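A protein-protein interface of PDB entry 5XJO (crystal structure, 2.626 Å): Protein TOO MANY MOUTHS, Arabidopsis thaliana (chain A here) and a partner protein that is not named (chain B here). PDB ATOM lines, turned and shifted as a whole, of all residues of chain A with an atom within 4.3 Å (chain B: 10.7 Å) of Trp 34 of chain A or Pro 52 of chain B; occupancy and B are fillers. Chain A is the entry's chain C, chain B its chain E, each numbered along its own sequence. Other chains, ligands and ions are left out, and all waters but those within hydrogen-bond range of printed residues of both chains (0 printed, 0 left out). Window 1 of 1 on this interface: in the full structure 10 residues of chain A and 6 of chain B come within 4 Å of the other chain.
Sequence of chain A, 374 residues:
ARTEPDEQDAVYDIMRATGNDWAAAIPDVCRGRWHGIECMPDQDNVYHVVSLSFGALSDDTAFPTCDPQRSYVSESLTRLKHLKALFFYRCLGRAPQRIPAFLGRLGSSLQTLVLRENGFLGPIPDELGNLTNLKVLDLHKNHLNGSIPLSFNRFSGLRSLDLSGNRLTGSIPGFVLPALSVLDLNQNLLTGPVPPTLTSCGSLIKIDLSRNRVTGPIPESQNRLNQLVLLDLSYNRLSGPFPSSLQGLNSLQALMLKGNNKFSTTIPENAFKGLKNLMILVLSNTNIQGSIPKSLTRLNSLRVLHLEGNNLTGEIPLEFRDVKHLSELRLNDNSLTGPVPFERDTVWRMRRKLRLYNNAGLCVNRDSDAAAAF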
ATOM      1  N   VAL A  11       6.094   1.629  10.842  1.00  0.00           N
ATOM      2  CA  VAL A  11       6.210   0.299  11.428  1.00  0.00           C
ATOM      3  C   VAL A  11       4.869  -0.147  11.991  1.00  0.00           C
ATOM      4  O   VAL A  11       4.375  -1.230  11.666  1.00  0.00           O
ATOM      5  CB  VAL A  11       7.313   0.293  12.499  1.00  0.00           C
ATOM      6  CG1 VAL A  11       7.334  -1.015  13.236  1.00  0.00           C
ATOM      7  CG2 VAL A  11       8.649   0.566  11.845  1.00  0.00           C
ATOM      8  N   MET A  15       2.728  -3.429  10.739  1.00  0.00           N
ATOM      9  CA  MET A  15       2.387  -4.505  11.637  1.00  0.00           C
ATOM     10  C   MET A  15       0.901  -4.710  11.779  1.00  0.00           C
ATOM     11  O   MET A  15       0.462  -5.769  12.112  1.00  0.00           O
ATOM     12  CB  MET A  15       3.087  -4.370  12.971  1.00  0.00           C
ATOM     13  CG  MET A  15       4.570  -4.108  12.854  1.00  0.00           C
ATOM     14  SD  MET A  15       5.672  -5.452  12.411  1.00  0.00           S
ATOM     15  CE  MET A  15       4.944  -6.826  13.237  1.00  0.00           C
ATOM     16  N   TRP A  22      -0.107  -5.896  18.475  1.00  0.00           N
ATOM     17  CA  TRP A  22       0.622  -5.771  19.726  1.00  0.00           C
ATOM     18  C   TRP A  22       1.824  -4.872  19.587  1.00  0.00           C
ATOM     19  O   TRP A  22       2.387  -4.454  20.603  1.00  0.00           O
ATOM     20  CB  TRP A  22       1.051  -7.160  20.232  1.00  0.00           C
ATOM     21  CG  TRP A  22       1.667  -7.997  19.159  1.00  0.00           C
ATOM     22  CD1 TRP A  22       1.040  -8.931  18.396  1.00  0.00           C
ATOM     23  CD2 TRP A  22       3.020  -7.925  18.684  1.00  0.00           C
ATOM     24  NE1 TRP A  22       1.919  -9.462  17.490  1.00  0.00           N
ATOM     25  CE2 TRP A  22       3.144  -8.862  17.648  1.00  0.00           C
ATOM     26  CE3 TRP A  22       4.140  -7.169  19.046  1.00  0.00           C
ATOM     27  CZ2 TRP A  22       4.341  -9.061  16.960  1.00  0.00           C
ATOM     28  CZ3 TRP A  22       5.329  -7.366  18.363  1.00  0.00           C
ATOM     29  CH2 TRP A  22       5.420  -8.302  17.337  1.00  0.00           C
ATOM     30  N   ILE A  26       3.761  -1.045  21.765  1.00  0.00           N
ATOM     31  CA  ILE A  26       5.173  -0.941  22.148  1.00  0.00           C
ATOM     32  C   ILE A  26       5.588   0.527  22.086  1.00  0.00           C
ATOM     33  O   ILE A  26       5.349   1.185  21.062  1.00  0.00           O
ATOM     34  CB  ILE A  26       6.047  -1.794  21.231  1.00  0.00           C
ATOM     35  CG1 ILE A  26       5.771  -3.286  21.446  1.00  0.00           C
ATOM     36  CG2 ILE A  26       7.531  -1.474  21.430  1.00  0.00           C
ATOM     37  CD1 ILE A  26       6.502  -4.181  20.457  1.00  0.00           C
ATOM     38  N   VAL A  29       9.908   1.134  19.192  1.00  0.00           N
ATOM     39  CA  VAL A  29      10.089  -0.059  18.376  1.00  0.00           C
ATOM     40  C   VAL A  29      11.504  -0.526  18.143  1.00  0.00           C
ATOM     41  O   VAL A  29      11.745  -1.709  18.068  1.00  0.00           O
ATOM     42  CB  VAL A  29       9.341   0.097  17.050  1.00  0.00           C
ATOM     43  CG1 VAL A  29      10.067  -0.597  15.934  1.00  0.00           C
ATOM     44  CG2 VAL A  29       7.931  -0.409  17.168  1.00  0.00           C
ATOM     45  N   GLY A  32      12.419  -1.544  21.863  1.00  0.00           N
ATOM     46  CA  GLY A  32      11.657  -2.717  22.211  1.00  0.00           C
ATOM     47  C   GLY A  32      11.517  -3.630  20.995  1.00  0.00           C
ATOM     48  O   GLY A  32      10.427  -3.794  20.504  1.00  0.00           O
ATOM     49  N   ARG A  33      12.598  -4.219  20.505  1.00  0.00           N
ATOM     50  CA  ARG A  33      12.515  -5.075  19.341  1.00  0.00           C
ATOM     51  C   ARG A  33      12.058  -6.472  19.568  1.00  0.00           C
ATOM     52  O   ARG A  33      12.065  -6.990  20.635  1.00  0.00           O
ATOM     53  CB  ARG A  33      13.803  -5.115  18.542  1.00  0.00           C
ATOM     54  CG  ARG A  33      14.687  -3.907  18.692  1.00  0.00           C
ATOM     55  CD  ARG A  33      16.141  -4.271  18.524  1.00  0.00           C
ATOM     56  NE  ARG A  33      16.359  -4.928  17.251  1.00  0.00           N
ATOM     57  CZ  ARG A  33      17.225  -5.896  17.040  1.00  0.00           C
ATOM     58  NH1 ARG A  33      17.986  -6.326  18.003  1.00  0.00           N
ATOM     59  NH2 ARG A  33      17.334  -6.422  15.855  1.00  0.00           N
ATOM     60  N   TRP A  34      11.624  -7.052  18.486  1.00  0.00           N
ATOM     61  CA  TRP A  34      11.206  -8.415  18.388  1.00  0.00           C
ATOM     62  C   TRP A  34      12.033  -9.016  17.250  1.00  0.00           C
ATOM     63  O   TRP A  34      12.580  -8.331  16.423  1.00  0.00           O
ATOM     64  CB  TRP A  34       9.732  -8.518  18.086  1.00  0.00           C
ATOM     65  CG  TRP A  34       9.344  -7.798  16.869  1.00  0.00           C
ATOM     66  CD1 TRP A  34       9.304  -8.295  15.635  1.00  0.00           C
ATOM     67  CD2 TRP A  34       8.944  -6.433  16.759  1.00  0.00           C
ATOM     68  NE1 TRP A  34       8.920  -7.348  14.754  1.00  0.00           N
ATOM     69  CE2 TRP A  34       8.690  -6.189  15.423  1.00  0.00           C
ATOM     70  CE3 TRP A  34       8.775  -5.401  17.662  1.00  0.00           C
ATOM     71  CZ2 TRP A  34       8.275  -4.968  14.969  1.00  0.00           C
ATOM     72  CZ3 TRP A  34       8.380  -4.197  17.198  1.00  0.00           C
ATOM     73  CH2 TRP A  34       8.131  -3.986  15.881  1.00  0.00           C
ATOM     74  N   HIS A  35      12.203 -10.310  17.250  1.00  0.00           N
ATOM     75  CA  HIS A  35      12.941 -10.913  16.163  1.00  0.00           C
ATOM     76  C   HIS A  35      12.173 -10.661  14.866  1.00  0.00           C
ATOM     77  O   HIS A  35      10.997 -11.021  14.749  1.00  0.00           O
ATOM     78  CB  HIS A  35      13.123 -12.396  16.414  1.00  0.00           C
ATOM     79  CG  HIS A  35      14.031 -13.037  15.428  1.00  0.00           C
ATOM     80  ND1 HIS A  35      15.337 -12.627  15.257  1.00  0.00           N
ATOM     81  CD2 HIS A  35      13.821 -14.035  14.543  1.00  0.00           C
ATOM     82  CE1 HIS A  35      15.892 -13.349  14.305  1.00  0.00           C
ATOM     83  NE2 HIS A  35      14.994 -14.206  13.852  1.00  0.00           N
ATOM     84  N   GLY A  36      12.802  -9.966  13.928  1.00  0.00           N
ATOM     85  CA  GLY A  36      12.083  -9.541  12.743  1.00  0.00           C
ATOM     86  C   GLY A  36      12.113  -8.051  12.469  1.00  0.00           C
ATOM     87  O   GLY A  36      11.503  -7.579  11.515  1.00  0.00           O
ATOM     88  N   ILE A  37      12.859  -7.312  13.279  1.00  0.00           N
ATOM     89  CA  ILE A  37      13.174  -5.914  13.017  1.00  0.00           C
ATOM     90  C   ILE A  37      14.578  -5.621  13.547  1.00  0.00           C
ATOM     91  O   ILE A  37      14.936  -6.026  14.659  1.00  0.00           O
ATOM     92  CB  ILE A  37      12.124  -4.974  13.639  1.00  0.00           C
ATOM     93  CG1 ILE A  37      12.549  -3.517  13.477  1.00  0.00           C
ATOM     94  CG2 ILE A  37      11.882  -5.329  15.087  1.00  0.00           C
ATOM     95  CD1 ILE A  37      11.404  -2.571  13.627  1.00  0.00           C
ATOM     96  N   PRO A  64       7.261 -12.576  13.032  1.00  0.00           N
ATOM     97  CA  PRO A  64       5.832 -12.312  13.208  1.00  0.00           C
ATOM     98  C   PRO A  64       4.969 -12.999  12.153  1.00  0.00           C
ATOM     99  O   PRO A  64       5.205 -12.878  10.961  1.00  0.00           O
ATOM    100  CB  PRO A  64       5.764 -10.788  13.108  1.00  0.00           C
ATOM    101  CG  PRO A  64       7.068 -10.332  13.622  1.00  0.00           C
ATOM    102  CD  PRO A  64       8.077 -11.381  13.308  1.00  0.00           C
ATOM    103  N   ARG B   4      25.222  -7.262  22.292  1.00  0.00           N
ATOM    104  CA  ARG B   4      24.567  -7.026  23.543  1.00  0.00           C
ATOM    105  C   ARG B   4      23.703  -8.197  23.855  1.00  0.00           C
ATOM    106  O   ARG B   4      23.359  -8.960  22.993  1.00  0.00           O
ATOM    107  CB  ARG B   4      23.640  -5.822  23.433  1.00  0.00           C
ATOM    108  CG  ARG B   4      24.313  -4.480  23.226  1.00  0.00           C
ATOM    109  CD  ARG B   4      23.291  -3.357  23.182  1.00  0.00           C
ATOM    110  NE  ARG B   4      23.913  -2.066  22.913  1.00  0.00           N
ATOM    111  CZ  ARG B   4      23.245  -0.937  22.709  1.00  0.00           C
ATOM    112  NH1 ARG B   4      21.923  -0.922  22.740  1.00  0.00           N
ATOM    113  NH2 ARG B   4      23.896   0.190  22.486  1.00  0.00           N
ATOM    114  N   LEU B   5      23.306  -8.310  25.099  1.00  0.00           N
ATOM    115  CA  LEU B   5      22.422  -9.358  25.516  1.00  0.00           C
ATOM    116  C   LEU B   5      21.024  -9.091  24.998  1.00  0.00           C
ATOM    117  O   LEU B   5      20.516  -8.043  25.214  1.00  0.00           O
ATOM    118  CB  LEU B   5      22.431  -9.361  27.018  1.00  0.00           C
ATOM    119  CG  LEU B   5      21.563 -10.366  27.714  1.00  0.00           C
ATOM    120  CD1 LEU B   5      22.146 -11.717  27.441  1.00  0.00           C
ATOM    121  CD2 LEU B   5      21.552 -10.075  29.195  1.00  0.00           C
ATOM    122  N   PRO B   6      20.389 -10.041  24.306  1.00  0.00           N
ATOM    123  CA  PRO B   6      19.046  -9.765  23.764  1.00  0.00           C
ATOM    124  C   PRO B   6      18.062  -9.362  24.849  1.00  0.00           C
ATOM    125  O   PRO B   6      18.005  -9.956  25.921  1.00  0.00           O
ATOM    126  CB  PRO B   6      18.647 -11.089  23.095  1.00  0.00           C
ATOM    127  CG  PRO B   6      19.894 -11.715  22.706  1.00  0.00           C
ATOM    128  CD  PRO B   6      20.994 -11.211  23.643  1.00  0.00           C
ATOM    129  N   ASP B   7      17.319  -8.300  24.571  1.00  0.00           N
ATOM    130  CA  ASP B   7      16.280  -7.785  25.450  1.00  0.00           C
ATOM    131  C   ASP B   7      14.953  -8.332  24.943  1.00  0.00           C
ATOM    132  O   ASP B   7      14.594  -8.126  23.778  1.00  0.00           O
ATOM    133  CB  ASP B   7      16.279  -6.255  25.465  1.00  0.00           C
ATOM    134  CG  ASP B   7      15.164  -5.674  26.323  1.00  0.00           C
ATOM    135  OD1 ASP B   7      15.314  -5.607  27.558  1.00  0.00           O
ATOM    136  OD2 ASP B   7      14.127  -5.284  25.758  1.00  0.00           O
ATOM    137  N   CYS B   8      14.276  -9.101  25.785  1.00  0.00           N
ATOM    138  CA  CYS B   8      13.059  -9.789  25.396  1.00  0.00           C
ATOM    139  C   CYS B   8      11.805  -9.009  25.751  1.00  0.00           C
ATOM    140  O   CYS B   8      10.702  -9.540  25.589  1.00  0.00           O
ATOM    141  CB  CYS B   8      12.983 -11.149  26.085  1.00  0.00           C
ATOM    142  SG  CYS B   8      14.144 -12.332  25.455  1.00  0.00           S
ATOM    143  N   SER B   9      11.940  -7.753  26.182  1.00  0.00           N
ATOM    144  CA  SER B   9      10.828  -7.084  26.857  1.00  0.00           C
ATOM    145  C   SER B   9       9.587  -6.977  25.973  1.00  0.00           C
ATOM    146  O   SER B   9       8.467  -6.933  26.491  1.00  0.00           O
ATOM    147  CB  SER B   9      11.281  -5.713  27.336  1.00  0.00           C
ATOM    148  OG  SER B   9      12.138  -5.864  28.456  1.00  0.00           O
ATOM    149  N   HIS B  10       9.749  -6.970  24.647  1.00  0.00           N
ATOM    150  CA  HIS B  10       8.607  -6.931  23.736  1.00  0.00           C
ATOM    151  C   HIS B  10       8.711  -7.985  22.637  1.00  0.00           C
ATOM    152  O   HIS B  10       8.167  -7.788  21.545  1.00  0.00           O
ATOM    153  CB  HIS B  10       8.441  -5.551  23.092  1.00  0.00           C
ATOM    154  CG  HIS B  10       7.992  -4.475  24.031  1.00  0.00           C
ATOM    155  ND1 HIS B  10       6.692  -4.374  24.479  1.00  0.00           N
ATOM    156  CD2 HIS B  10       8.661  -3.431  24.581  1.00  0.00           C
ATOM    157  CE1 HIS B  10       6.581  -3.326  25.277  1.00  0.00           C
ATOM    158  NE2 HIS B  10       7.761  -2.736  25.353  1.00  0.00           N
ATOM    159  N   ALA B  11       9.383  -9.112  22.904  1.00  0.00           N
ATOM    160  CA  ALA B  11       9.686 -10.101  21.868  1.00  0.00           C
ATOM    161  C   ALA B  11       8.714 -11.278  21.809  1.00  0.00           C
ATOM    162  O   ALA B  11       8.872 -12.141  20.937  1.00  0.00           O
ATOM    163  CB  ALA B  11      11.115 -10.638  22.050  1.00  0.00           C
ATOM    164  N   CYS B  12       7.688 -11.324  22.659  1.00  0.00           N
ATOM    165  CA  CYS B  12       6.736 -12.434  22.663  1.00  0.00           C
ATOM    166  C   CYS B  12       5.363 -11.966  22.193  1.00  0.00           C
ATOM    167  O   CYS B  12       4.322 -12.448  22.655  1.00  0.00           O
ATOM    168  CB  CYS B  12       6.633 -13.088  24.046  1.00  0.00           C
ATOM    169  SG  CYS B  12       8.183 -13.681  24.843  1.00  0.00           S
ATOM    170  N   GLY B  13       5.370 -11.060  21.217  1.00  0.00           N
ATOM    171  CA  GLY B  13       4.141 -10.536  20.669  1.00  0.00           C
ATOM    172  C   GLY B  13       3.339  -9.862  21.774  1.00  0.00           C
ATOM    173  O   GLY B  13       3.772  -8.928  22.442  1.00  0.00           O
ATOM    174  N   SER B  14       2.178 -10.460  21.983  1.00  0.00           N
ATOM    175  CA  SER B  14       1.163 -10.063  22.958  1.00  0.00           C
ATOM    176  C   SER B  14       1.064 -11.041  24.139  1.00  0.00           C
ATOM    177  O   SER B  14      -0.004 -11.176  24.743  1.00  0.00           O
ATOM    178  CB  SER B  14      -0.136  -9.910  22.129  1.00  0.00           C
ATOM    179  OG  SER B  14      -0.978 -11.069  22.087  1.00  0.00           O
ATOM    180  N   CYS B  15       2.183 -11.679  24.498  1.00  0.00           N
ATOM    181  CA  CYS B  15       2.429 -12.306  25.790  1.00  0.00           C
ATOM    182  C   CYS B  15       3.316 -11.390  26.633  1.00  0.00           C
ATOM    183  O   CYS B  15       4.360 -10.923  26.152  1.00  0.00           O
ATOM    184  CB  CYS B  15       3.095 -13.674  25.611  1.00  0.00           C
ATOM    185  SG  CYS B  15       2.943 -14.825  27.021  1.00  0.00           S
ATOM    186  N   CYS B  18       7.579 -11.590  29.194  1.00  0.00           N
ATOM    187  CA  CYS B  18       8.527 -12.067  28.196  1.00  0.00           C
ATOM    188  C   CYS B  18       9.943 -11.828  28.713  1.00  0.00           C
ATOM    189  O   CYS B  18      10.398 -10.682  28.795  1.00  0.00           O
ATOM    190  CB  CYS B  18       8.289 -11.356  26.863  1.00  0.00           C
ATOM    191  SG  CYS B  18       9.205 -12.024  25.438  1.00  0.00           S
ATOM    192  N   ARG B  19      10.652 -12.919  29.020  1.00  0.00           N
ATOM    193  CA  ARG B  19      11.928 -12.866  29.723  1.00  0.00           C
ATOM    194  C   ARG B  19      12.908 -13.847  29.099  1.00  0.00           C
ATOM    195  O   ARG B  19      12.517 -14.876  28.548  1.00  0.00           O
ATOM    196  CB  ARG B  19      11.766 -13.170  31.209  1.00  0.00           C
ATOM    197  CG  ARG B  19      10.632 -12.421  31.889  1.00  0.00           C
ATOM    198  CD  ARG B  19      11.172 -11.176  32.590  1.00  0.00           C
ATOM    199  NE  ARG B  19      10.203 -10.668  33.546  1.00  0.00           N
ATOM    200  CZ  ARG B  19       9.981 -11.206  34.740  1.00  0.00           C
ATOM    201  NH1 ARG B  19       9.065 -10.687  35.552  1.00  0.00           N
ATOM    202  NH2 ARG B  19      10.674 -12.263  35.128  1.00  0.00           N
ATOM    203  N   LEU B  20      14.188 -13.498  29.162  1.00  0.00           N
ATOM    204  CA  LEU B  20      15.240 -14.290  28.538  1.00  0.00           C
ATOM    205  C   LEU B  20      15.618 -15.515  29.364  1.00  0.00           C
ATOM    206  O   LEU B  20      15.712 -15.448  30.596  1.00  0.00           O
ATOM    207  CB  LEU B  20      16.463 -13.412  28.327  1.00  0.00           C
ATOM    208  CG  LEU B  20      17.787 -13.970  27.825  1.00  0.00           C
ATOM    209  CD1 LEU B  20      17.671 -14.978  26.700  1.00  0.00           C
ATOM    210  CD2 LEU B  20      18.460 -12.755  27.285  1.00  0.00           C
ATOM    211  N   VAL B  21      15.838 -16.642  28.670  1.00  0.00           N
ATOM    212  CA  VAL B  21      16.208 -17.927  29.277  1.00  0.00           C
ATOM    213  C   VAL B  21      17.148 -18.652  28.316  1.00  0.00           C
ATOM    214  O   VAL B  21      16.960 -18.623  27.094  1.00  0.00           O
ATOM    215  CB  VAL B  21      14.982 -18.812  29.639  1.00  0.00           C
ATOM    216  CG1 VAL B  21      13.917 -18.036  30.438  1.00  0.00           C
ATOM    217  CG2 VAL B  21      14.374 -19.477  28.410  1.00  0.00           C
ATOM    218  N   TYR B  40      20.401 -18.310  23.180  1.00  0.00           N
ATOM    219  CA  TYR B  40      19.365 -17.659  23.985  1.00  0.00           C
ATOM    220  C   TYR B  40      17.977 -17.798  23.356  1.00  0.00           C
ATOM    221  O   TYR B  40      17.837 -17.846  22.136  1.00  0.00           O
ATOM    222  CB  TYR B  40      19.666 -16.168  24.164  1.00  0.00           C
ATOM    223  CG  TYR B  40      20.991 -15.784  24.787  1.00  0.00           C
ATOM    224  CD1 TYR B  40      21.063 -15.469  26.144  1.00  0.00           C
ATOM    225  CD2 TYR B  40      22.146 -15.638  24.014  1.00  0.00           C
ATOM    226  CE1 TYR B  40      22.254 -15.068  26.743  1.00  0.00           C
ATOM    227  CE2 TYR B  40      23.363 -15.255  24.600  1.00  0.00           C
ATOM    228  CZ  TYR B  40      23.412 -14.960  25.970  1.00  0.00           C
ATOM    229  OH  TYR B  40      24.614 -14.561  26.581  1.00  0.00           O
ATOM    230  N   LYS B  41      16.945 -17.846  24.199  1.00  0.00           N
ATOM    231  CA  LYS B  41      15.575 -17.700  23.705  1.00  0.00           C
ATOM    232  C   LYS B  41      14.798 -16.775  24.638  1.00  0.00           C
ATOM    233  O   LYS B  41      15.233 -16.476  25.757  1.00  0.00           O
ATOM    234  CB  LYS B  41      14.856 -19.060  23.561  1.00  0.00           C
ATOM    235  CG  LYS B  41      15.627 -20.169  22.803  1.00  0.00           C
ATOM    236  CD  LYS B  41      15.732 -19.969  21.280  1.00  0.00           C
ATOM    237  CE  LYS B  41      16.638 -21.053  20.638  1.00  0.00           C
ATOM    238  NZ  LYS B  41      16.887 -20.930  19.159  1.00  0.00           N
ATOM    239  N   CYS B  42      13.636 -16.310  24.171  1.00  0.00           N
ATOM    240  CA  CYS B  42      12.688 -15.576  25.014  1.00  0.00           C
ATOM    241  C   CYS B  42      11.541 -16.498  25.403  1.00  0.00           C
ATOM    242  O   CYS B  42      11.087 -17.305  24.596  1.00  0.00           O
ATOM    243  CB  CYS B  42      12.106 -14.340  24.309  1.00  0.00           C
ATOM    244  SG  CYS B  42      13.255 -13.036  23.767  1.00  0.00           S
ATOM    245  N   MET B  43      11.032 -16.337  26.620  1.00  0.00           N
ATOM    246  CA  MET B  43      10.009 -17.227  27.152  1.00  0.00           C
ATOM    247  C   MET B  43       8.917 -16.439  27.865  1.00  0.00           C
ATOM    248  O   MET B  43       9.197 -15.456  28.563  1.00  0.00           O
ATOM    249  CB  MET B  43      10.617 -18.240  28.121  1.00  0.00           C
ATOM    250  CG  MET B  43       9.700 -19.389  28.468  1.00  0.00           C
ATOM    251  SD  MET B  43      10.731 -20.838  28.542  1.00  0.00           S
ATOM    252  CE  MET B  43      11.296 -20.863  26.855  1.00  0.00           C
ATOM    253  N   SER B  48       8.023 -20.716  24.055  1.00  0.00           N
ATOM    254  CA  SER B  48       9.293 -20.226  23.530  1.00  0.00           C
ATOM    255  C   SER B  48       9.071 -19.269  22.365  1.00  0.00           C
ATOM    256  O   SER B  48       8.120 -19.412  21.598  1.00  0.00           O
ATOM    257  CB  SER B  48      10.187 -21.383  23.057  1.00  0.00           C
ATOM    258  OG  SER B  48      10.786 -22.076  24.139  1.00  0.00           O
ATOM    259  N   TYR B  49       9.965 -18.296  22.243  1.00  0.00           N
ATOM    260  CA  TYR B  49      10.020 -17.319  21.165  1.00  0.00           C
ATOM    261  C   TYR B  49      11.484 -17.031  20.875  1.00  0.00           C
ATOM    262  O   TYR B  49      12.347 -17.280  21.725  1.00  0.00           O
ATOM    263  CB  TYR B  49       9.309 -16.000  21.503  1.00  0.00           C
ATOM    264  CG  TYR B  49       7.858 -16.109  21.854  1.00  0.00           C
ATOM    265  CD1 TYR B  49       7.452 -16.475  23.126  1.00  0.00           C
ATOM    266  CD2 TYR B  49       6.891 -15.820  20.913  1.00  0.00           C
ATOM    267  CE1 TYR B  49       6.117 -16.557  23.441  1.00  0.00           C
ATOM    268  CE2 TYR B  49       5.566 -15.902  21.214  1.00  0.00           C
ATOM    269  CZ  TYR B  49       5.178 -16.267  22.471  1.00  0.00           C
ATOM    270  OH  TYR B  49       3.839 -16.329  22.729  1.00  0.00           O
ATOM    271  N   PRO B  50      11.803 -16.533  19.680  1.00  0.00           N
ATOM    272  CA  PRO B  50      13.194 -16.181  19.389  1.00  0.00           C
ATOM    273  C   PRO B  50      13.562 -14.779  19.866  1.00  0.00           C
ATOM    274  O   PRO B  50      12.753 -13.850  19.885  1.00  0.00           O
ATOM    275  CB  PRO B  50      13.268 -16.292  17.859  1.00  0.00           C
ATOM    276  CG  PRO B  50      11.831 -16.541  17.378  1.00  0.00           C
ATOM    277  CD  PRO B  50      10.926 -16.303  18.512  1.00  0.00           C
ATOM    278  N   VAL B  51      14.834 -14.640  20.238  1.00  0.00           N
ATOM    279  CA  VAL B  51      15.405 -13.379  20.712  1.00  0.00           C
ATOM    280  C   VAL B  51      15.436 -12.366  19.573  1.00  0.00           C
ATOM    281  O   VAL B  51      15.610 -12.769  18.420  1.00  0.00           O
ATOM    282  CB  VAL B  51      16.814 -13.612  21.285  1.00  0.00           C
ATOM    283  CG1 VAL B  51      16.783 -14.744  22.287  1.00  0.00           C
ATOM    284  CG2 VAL B  51      17.837 -13.907  20.180  1.00  0.00           C
ATOM    285  N   PRO B  52      15.248 -11.054  19.827  1.00  0.00           N
ATOM    286  CA  PRO B  52      15.401 -10.038  18.758  1.00  0.00           C
ATOM    287  C   PRO B  52      16.757 -10.120  18.082  1.00  0.00           C
ATOM    288  O   PRO B  52      16.772 -10.567  16.937  1.00  0.00           O
ATOM    289  CB  PRO B  52      15.244  -8.695  19.486  1.00  0.00           C
ATOM    290  CG  PRO B  52      14.433  -9.020  20.689  1.00  0.00           C
ATOM    291  CD  PRO B  52      14.677 -10.478  21.057  1.00  0.00           C
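Printed residues of chain B that touch a printed residue of chain A: His 10, Gly 13, Ser 14, Pro 50, Val 51 and Pro 52. Hydrophobic or aromatic side chains of chain B within 4 Å of the printed part of chain A: His 10 and Pro 52. Printed residues of chain A that touch a printed residue of chain B: Trp 22, Ile 26, Gly 32, Arg 33, Trp 34 and His 35. Among the printed residues, 10 pairs touch across the chains. Among the printed residues, no Asp or Glu carboxylate lies within 4 Å of a Lys or Arg side-chain nitrogen of the other chain.
The backbone carbonyl oxygen (O) of Val 51 of chain B sits at hydrogen-bond distance from a ring nitrogen (ND1) of His 35 of chain A, at 3.2 Å. ND1 of His 35 of chain A is in hydrogen-bond range of O of Pro 52 of chain B (3.0 Å).
The guanidinium group (NH2) of Arg 33 of chain A sits at hydrogen-bond distance from the backbone carbonyl oxygen (O) of Ile 37 of chain A, 2.7 Å away. The side-chain sulfur (SG) of Cys 8 of chain B is disulfide-bonded to the side-chain sulfur (SG) of Cys 42 of chain B (2.0 Å). SG of Cys 12 of chain B is disulfide-bonded to SG of Cys 18 of chain B, 2.0 Å away.
Trp 22 of chain A touches Gly 13 of chain B. Ser 14 of chain B touches Trp 22 of chain A. Ile 26 of chain A touches His 10 of chain B. Gly 32 of chain A touches His 10 of chain B (O to CB, 3.7 Å). Arg 33 of chain A touches Pro 52 of chain B. Trp 34 of chain A touches His 10 of chain B (CB to O, 3.9 Å). CA of Pro 52 of chain B touches C of Trp 34 of chain A, 3.8 Å away. Pro 50 of chain B touches His 35 of chain A (O to CB, 3.8 Å).
Of the printed residues of chain B, Trp 34 of chain A touches His 10 and Pro 52. No residue of chain B comes within 4 Å of Val 29 of chain A. Arg 33 of chain A touches one residue of chain B. No residue of chain B comes within 4 Å of Gly 36 of chain A. No residue of chain B comes within 4 Å of Ile 37 of chain A. Printed residues of chain A within 4 Å of Gly 13 of chain B: Trp 22. Of the printed residues of chain A, Ser 14 of chain B touches Trp 22 (3.5 Å). Ser 48 of chain B touches none of the printed residues of chain A. The nearest printed residue of chain B that does not touch Ile 26 of chain A is Gly 13 of chain B (5.8 Å).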
